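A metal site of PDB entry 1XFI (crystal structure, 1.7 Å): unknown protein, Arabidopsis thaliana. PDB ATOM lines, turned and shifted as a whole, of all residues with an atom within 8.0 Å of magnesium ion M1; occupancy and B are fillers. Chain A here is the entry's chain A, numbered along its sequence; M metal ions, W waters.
Magnesium ion M1 is bound by water W1 (2.0 Å), water W3 (2.1 Å), water W2 (2.1 Å), the side-chain carboxylate (OD1) of Asp 256 (2.1 Å), the side-chain amide oxygen (OD1) of Asn 221 (2.1 Å) and the side-chain carboxylate (OD1) of Asp 220 (2.2 Å).
Magnesium ion M1 has six donor atoms within binding distance.
Within 4 Å of magnesium ion M1: Asp 220, Asn 221 and Asp 256.
The nearest printed residue that does not touch magnesium ion M1 is Asn 255 (4.2 Å).
Water W2 bridges the side-chain carboxylate (OD2) of Asp 220 (2.8 Å) and the side-chain amide nitrogen (ND2) of Asn 221 (3.4 Å).
The side-chain carboxylate (OD1) of Asp 220 sits close to the guanidinium group (NH1) of Arg 322 (3.2 Å).
The backbone NH (N) of Asn 221 is in hydrogen-bond range of the side-chain carboxylate (OD2) of Asp 225 (3.0 Å).
The side-chain amide oxygen (OD1) of Asn 255 lies close to the side-chain amide oxygen (OD1) of Asn 221 (3.5 Å).
The backbone carbonyl oxygen (O) of Asp 220 is in hydrogen-bond range of the backbone NH (N) of Ile 257.
N of Asp 220 lies within hydrogen-bond range of OE1 of Glu 318.
The side-chain carboxylate of Asp 256 is in salt-bridge range of the guanidinium group of Arg 322.
The side-chain carboxylate (OD2) of Asp 220 is in hydrogen-bond range of the side-chain amide nitrogen (ND2) of Asn 163.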
ATOM      1  N   ASN A 163     -20.618  34.109  -4.320  1.00  0.00           N
ATOM      2  CA  ASN A 163     -21.188  33.110  -3.453  1.00  0.00           C
ATOM      3  C   ASN A 163     -22.635  33.525  -3.103  1.00  0.00           C
ATOM      4  O   ASN A 163     -23.439  32.675  -2.710  1.00  0.00           O
ATOM      5  CB  ASN A 163     -20.153  32.880  -2.295  1.00  0.00           C
ATOM      6  CG  ASN A 163     -20.412  31.673  -1.458  1.00  0.00           C
ATOM      7  OD1 ASN A 163     -20.353  31.820  -0.229  1.00  0.00           O
ATOM      8  ND2 ASN A 163     -20.664  30.433  -2.089  1.00  0.00           N
ATOM      9  N   VAL A 219     -14.850  23.807  -3.727  1.00  0.00           N
ATOM     10  CA  VAL A 219     -15.771  24.747  -4.329  1.00  0.00           C
ATOM     11  C   VAL A 219     -17.232  24.507  -3.998  1.00  0.00           C
ATOM     12  O   VAL A 219     -17.657  23.468  -3.512  1.00  0.00           O
ATOM     13  CB  VAL A 219     -15.540  24.831  -5.847  1.00  0.00           C
ATOM     14  CG1 VAL A 219     -14.146  25.219  -6.140  1.00  0.00           C
ATOM     15  CG2 VAL A 219     -15.939  23.503  -6.569  1.00  0.00           C
ATOM     16  N   ASP A 220     -18.048  25.483  -4.375  1.00  0.00           N
ATOM     17  CA  ASP A 220     -19.457  25.514  -3.957  1.00  0.00           C
ATOM     18  C   ASP A 220     -20.374  25.610  -5.146  1.00  0.00           C
ATOM     19  O   ASP A 220     -20.672  24.592  -5.766  1.00  0.00           O
ATOM     20  CB  ASP A 220     -19.666  26.675  -2.966  1.00  0.00           C
ATOM     21  CG  ASP A 220     -21.099  26.685  -2.341  1.00  0.00           C
ATOM     22  OD1 ASP A 220     -21.941  25.798  -2.639  1.00  0.00           O
ATOM     23  OD2 ASP A 220     -21.326  27.585  -1.489  1.00  0.00           O
ATOM     24  N   ASN A 221     -20.880  26.788  -5.465  1.00  0.00           N
ATOM     25  CA  ASN A 221     -21.942  26.905  -6.436  1.00  0.00           C
ATOM     26  C   ASN A 221     -21.465  27.017  -7.891  1.00  0.00           C
ATOM     27  O   ASN A 221     -20.321  27.417  -8.177  1.00  0.00           O
ATOM     28  CB  ASN A 221     -22.808  28.162  -6.143  1.00  0.00           C
ATOM     29  CG  ASN A 221     -23.568  28.072  -4.893  1.00  0.00           C
ATOM     30  OD1 ASN A 221     -23.925  27.007  -4.476  1.00  0.00           O
ATOM     31  ND2 ASN A 221     -23.877  29.212  -4.302  1.00  0.00           N
ATOM     32  N   SER A 222     -22.368  26.655  -8.791  1.00  0.00           N
ATOM     33  CA  SER A 222     -22.216  26.909 -10.215  1.00  0.00           C
ATOM     34  C   SER A 222     -22.292  28.388 -10.544  1.00  0.00           C
ATOM     35  O   SER A 222     -22.364  29.243  -9.660  1.00  0.00           O
ATOM     36  CB  SER A 222     -23.319  26.175 -10.976  1.00  0.00           C
ATOM     37  OG  SER A 222     -23.230  24.792 -10.789  1.00  0.00           O
ATOM     38  N   ASP A 225     -20.304  31.959  -9.108  1.00  0.00           N
ATOM     39  CA  ASP A 225     -19.481  31.571  -8.007  1.00  0.00           C
ATOM     40  C   ASP A 225     -18.236  30.904  -8.551  1.00  0.00           C
ATOM     41  O   ASP A 225     -17.166  31.434  -8.386  1.00  0.00           O
ATOM     42  CB  ASP A 225     -20.287  30.629  -7.094  1.00  0.00           C
ATOM     43  CG  ASP A 225     -19.555  30.259  -5.810  1.00  0.00           C
ATOM     44  OD1 ASP A 225     -18.315  30.463  -5.774  1.00  0.00           O
ATOM     45  OD2 ASP A 225     -20.250  29.712  -4.889  1.00  0.00           O
ATOM     46  N   SER A 253     -25.989  18.442  -5.885  1.00  0.00           N
ATOM     47  CA  SER A 253     -26.697  18.810  -4.673  1.00  0.00           C
ATOM     48  C   SER A 253     -27.036  20.281  -4.837  1.00  0.00           C
ATOM     49  O   SER A 253     -26.131  21.081  -4.994  1.00  0.00           O
ATOM     50  CB  SER A 253     -25.792  18.581  -3.457  1.00  0.00           C
ATOM     51  OG  SER A 253     -26.433  18.994  -2.263  1.00  0.00           O
ATOM     52  N   ILE A 254     -28.325  20.634  -4.812  1.00  0.00           N
ATOM     53  CA  ILE A 254     -28.765  22.002  -5.041  1.00  0.00           C
ATOM     54  C   ILE A 254     -28.113  22.496  -6.367  1.00  0.00           C
ATOM     55  O   ILE A 254     -28.099  21.738  -7.361  1.00  0.00           O
ATOM     56  CB  ILE A 254     -28.484  22.946  -3.854  1.00  0.00           C
ATOM     57  CG1 ILE A 254     -28.748  22.264  -2.507  1.00  0.00           C
ATOM     58  CG2 ILE A 254     -29.422  24.149  -3.919  1.00  0.00           C
ATOM     59  CD1 ILE A 254     -28.396  23.179  -1.322  1.00  0.00           C
ATOM     60  N   ASN A 255     -27.563  23.701  -6.377  1.00  0.00           N
ATOM     61  CA  ASN A 255     -26.903  24.227  -7.580  1.00  0.00           C
ATOM     62  C   ASN A 255     -25.382  24.099  -7.519  1.00  0.00           C
ATOM     63  O   ASN A 255     -24.662  24.764  -8.266  1.00  0.00           O
ATOM     64  CB  ASN A 255     -27.372  25.672  -7.883  1.00  0.00           C
ATOM     65  CG  ASN A 255     -26.964  26.645  -6.805  1.00  0.00           C
ATOM     66  OD1 ASN A 255     -27.168  26.376  -5.612  1.00  0.00           O
ATOM     67  ND2 ASN A 255     -26.389  27.750  -7.206  1.00  0.00           N
ATOM     68  N   ASP A 256     -24.871  23.236  -6.629  1.00  0.00           N
ATOM     69  CA  ASP A 256     -23.478  23.108  -6.488  1.00  0.00           C
ATOM     70  C   ASP A 256     -22.838  22.474  -7.715  1.00  0.00           C
ATOM     71  O   ASP A 256     -23.436  21.616  -8.377  1.00  0.00           O
ATOM     72  CB  ASP A 256     -23.111  22.304  -5.257  1.00  0.00           C
ATOM     73  CG  ASP A 256     -23.468  23.038  -3.969  1.00  0.00           C
ATOM     74  OD1 ASP A 256     -24.038  24.139  -4.105  1.00  0.00           O
ATOM     75  OD2 ASP A 256     -23.241  22.489  -2.886  1.00  0.00           O
ATOM     76  N   ILE A 257     -21.640  22.908  -8.010  1.00  0.00           N
ATOM     77  CA  ILE A 257     -20.926  22.450  -9.202  1.00  0.00           C
ATOM     78  C   ILE A 257     -20.327  21.080  -8.921  1.00  0.00           C
ATOM     79  O   ILE A 257     -19.831  20.850  -7.836  1.00  0.00           O
ATOM     80  CB  ILE A 257     -19.812  23.521  -9.577  1.00  0.00           C
ATOM     81  CG1 ILE A 257     -19.071  23.164 -10.862  1.00  0.00           C
ATOM     82  CG2 ILE A 257     -18.811  23.746  -8.496  1.00  0.00           C
ATOM     83  CD1 ILE A 257     -19.841  23.357 -12.040  1.00  0.00           C
ATOM     84  N   LEU A 293     -23.339  16.253  -1.074  1.00  0.00           N
ATOM     85  CA  LEU A 293     -24.157  17.129  -0.245  1.00  0.00           C
ATOM     86  C   LEU A 293     -23.724  18.575  -0.456  1.00  0.00           C
ATOM     87  O   LEU A 293     -22.726  18.842  -1.092  1.00  0.00           O
ATOM     88  CB  LEU A 293     -23.969  16.786   1.241  1.00  0.00           C
ATOM     89  CG  LEU A 293     -24.305  15.322   1.615  1.00  0.00           C
ATOM     90  CD1 LEU A 293     -23.921  15.184   3.108  1.00  0.00           C
ATOM     91  CD2 LEU A 293     -25.742  15.005   1.359  1.00  0.00           C
ATOM     92  N   PRO A 294     -24.505  19.526   0.125  1.00  0.00           N
ATOM     93  CA  PRO A 294     -24.040  20.920   0.137  1.00  0.00           C
ATOM     94  C   PRO A 294     -23.179  21.331   1.313  1.00  0.00           C
ATOM     95  O   PRO A 294     -22.805  22.516   1.420  1.00  0.00           O
ATOM     96  CB  PRO A 294     -25.367  21.683   0.199  1.00  0.00           C
ATOM     97  CG  PRO A 294     -26.287  20.819   0.873  1.00  0.00           C
ATOM     98  CD  PRO A 294     -25.862  19.405   0.637  1.00  0.00           C
ATOM     99  N   VAL A 295     -22.930  20.376   2.208  1.00  0.00           N
ATOM    100  CA  VAL A 295     -21.990  20.487   3.266  1.00  0.00           C
ATOM    101  C   VAL A 295     -20.984  19.340   3.039  1.00  0.00           C
ATOM    102  O   VAL A 295     -21.188  18.556   2.138  1.00  0.00           O
ATOM    103  CB  VAL A 295     -22.644  20.299   4.650  1.00  0.00           C
ATOM    104  CG1 VAL A 295     -23.701  21.387   4.903  1.00  0.00           C
ATOM    105  CG2 VAL A 295     -23.260  18.958   4.781  1.00  0.00           C
ATOM    106  N   GLU A 318     -14.810  26.722   0.700  1.00  0.00           N
ATOM    107  CA  GLU A 318     -15.667  27.815   0.266  1.00  0.00           C
ATOM    108  C   GLU A 318     -17.135  27.563   0.547  1.00  0.00           C
ATOM    109  O   GLU A 318     -17.697  26.461   0.278  1.00  0.00           O
ATOM    110  CB  GLU A 318     -15.532  28.040  -1.245  1.00  0.00           C
ATOM    111  CG  GLU A 318     -16.215  29.322  -1.702  1.00  0.00           C
ATOM    112  CD  GLU A 318     -16.768  29.294  -3.112  1.00  0.00           C
ATOM    113  OE1 GLU A 318     -16.704  28.262  -3.801  1.00  0.00           O
ATOM    114  OE2 GLU A 318     -17.286  30.388  -3.472  1.00  0.00           O
ATOM    115  N   GLY A 319     -17.814  28.633   0.972  1.00  0.00           N
ATOM    116  CA  GLY A 319     -19.239  28.620   1.105  1.00  0.00           C
ATOM    117  C   GLY A 319     -19.751  28.279   2.465  1.00  0.00           C
ATOM    118  O   GLY A 319     -19.043  27.710   3.283  1.00  0.00           O
ATOM    119  N   MET A 320     -20.970  28.723   2.762  1.00  0.00           N
ATOM    120  CA  MET A 320     -21.525  28.523   4.072  1.00  0.00           C
ATOM    121  C   MET A 320     -21.657  27.053   4.401  1.00  0.00           C
ATOM    122  O   MET A 320     -21.453  26.676   5.529  1.00  0.00           O
ATOM    123  CB  MET A 320     -22.924  29.156   4.165  1.00  0.00           C
ATOM    124  CG  MET A 320     -23.616  28.931   5.486  1.00  0.00           C
ATOM    125  SD  MET A 320     -25.205  29.864   5.577  1.00  0.00           S
ATOM    126  CE  MET A 320     -26.115  29.069   4.296  1.00  0.00           C
ATOM    127  N   GLY A 321     -22.079  26.235   3.448  1.00  0.00           N
ATOM    128  CA  GLY A 321     -22.308  24.811   3.809  1.00  0.00           C
ATOM    129  C   GLY A 321     -21.040  24.063   4.174  1.00  0.00           C
ATOM    130  O   GLY A 321     -20.961  23.482   5.241  1.00  0.00           O
ATOM    131  N   ARG A 322     -20.055  24.138   3.300  1.00  0.00           N
ATOM    132  CA  ARG A 322     -18.773  23.435   3.501  1.00  0.00           C
ATOM    133  C   ARG A 322     -17.775  24.065   4.481  1.00  0.00           C
ATOM    134  O   ARG A 322     -16.969  23.330   5.083  1.00  0.00           O
ATOM    135  CB  ARG A 322     -18.057  23.238   2.130  1.00  0.00           C
ATOM    136  CG  ARG A 322     -18.842  22.329   1.238  1.00  0.00           C
ATOM    137  CD  ARG A 322     -18.258  22.343  -0.172  1.00  0.00           C
ATOM    138  NE  ARG A 322     -19.021  21.547  -1.080  1.00  0.00           N
ATOM    139  CZ  ARG A 322     -20.165  21.926  -1.655  1.00  0.00           C
ATOM    140  NH1 ARG A 322     -20.671  23.105  -1.345  1.00  0.00           N
ATOM    141  NH2 ARG A 322     -20.793  21.117  -2.496  1.00  0.00           N
ATOM    142  N   LYS A 343     -25.789  33.069   4.735  1.00  0.00           N
ATOM    143  CA  LYS A 343     -27.101  33.212   4.082  1.00  0.00           C
ATOM    144  C   LYS A 343     -28.298  32.634   4.897  1.00  0.00           C
ATOM    145  O   LYS A 343     -29.410  32.610   4.399  1.00  0.00           O
ATOM    146  CB  LYS A 343     -27.052  32.571   2.694  1.00  0.00           C
ATOM    147  CG  LYS A 343     -25.976  33.187   1.799  1.00  0.00           C
ATOM    148  CD  LYS A 343     -25.808  32.426   0.489  1.00  0.00           C
ATOM    149  CE  LYS A 343     -26.913  32.746  -0.492  1.00  0.00           C
ATOM    150  NZ  LYS A 343     -26.933  34.215  -0.798  1.00  0.00           N
HETATM  151 MG    MG M   1     -24.115  25.775  -2.765  1.00  0.00          MG
HETATM  152 MG    MG M   2     -27.376  23.756   3.808  1.00  0.00          MG
HETATM  153  O   HOH W   1     -24.189  24.545  -1.218  1.00  0.00           O
HETATM  154  O   HOH W   2     -24.072  27.414  -1.468  1.00  0.00           O
HETATM  155  O   HOH W   3     -26.142  25.863  -3.085  1.00  0.00           O
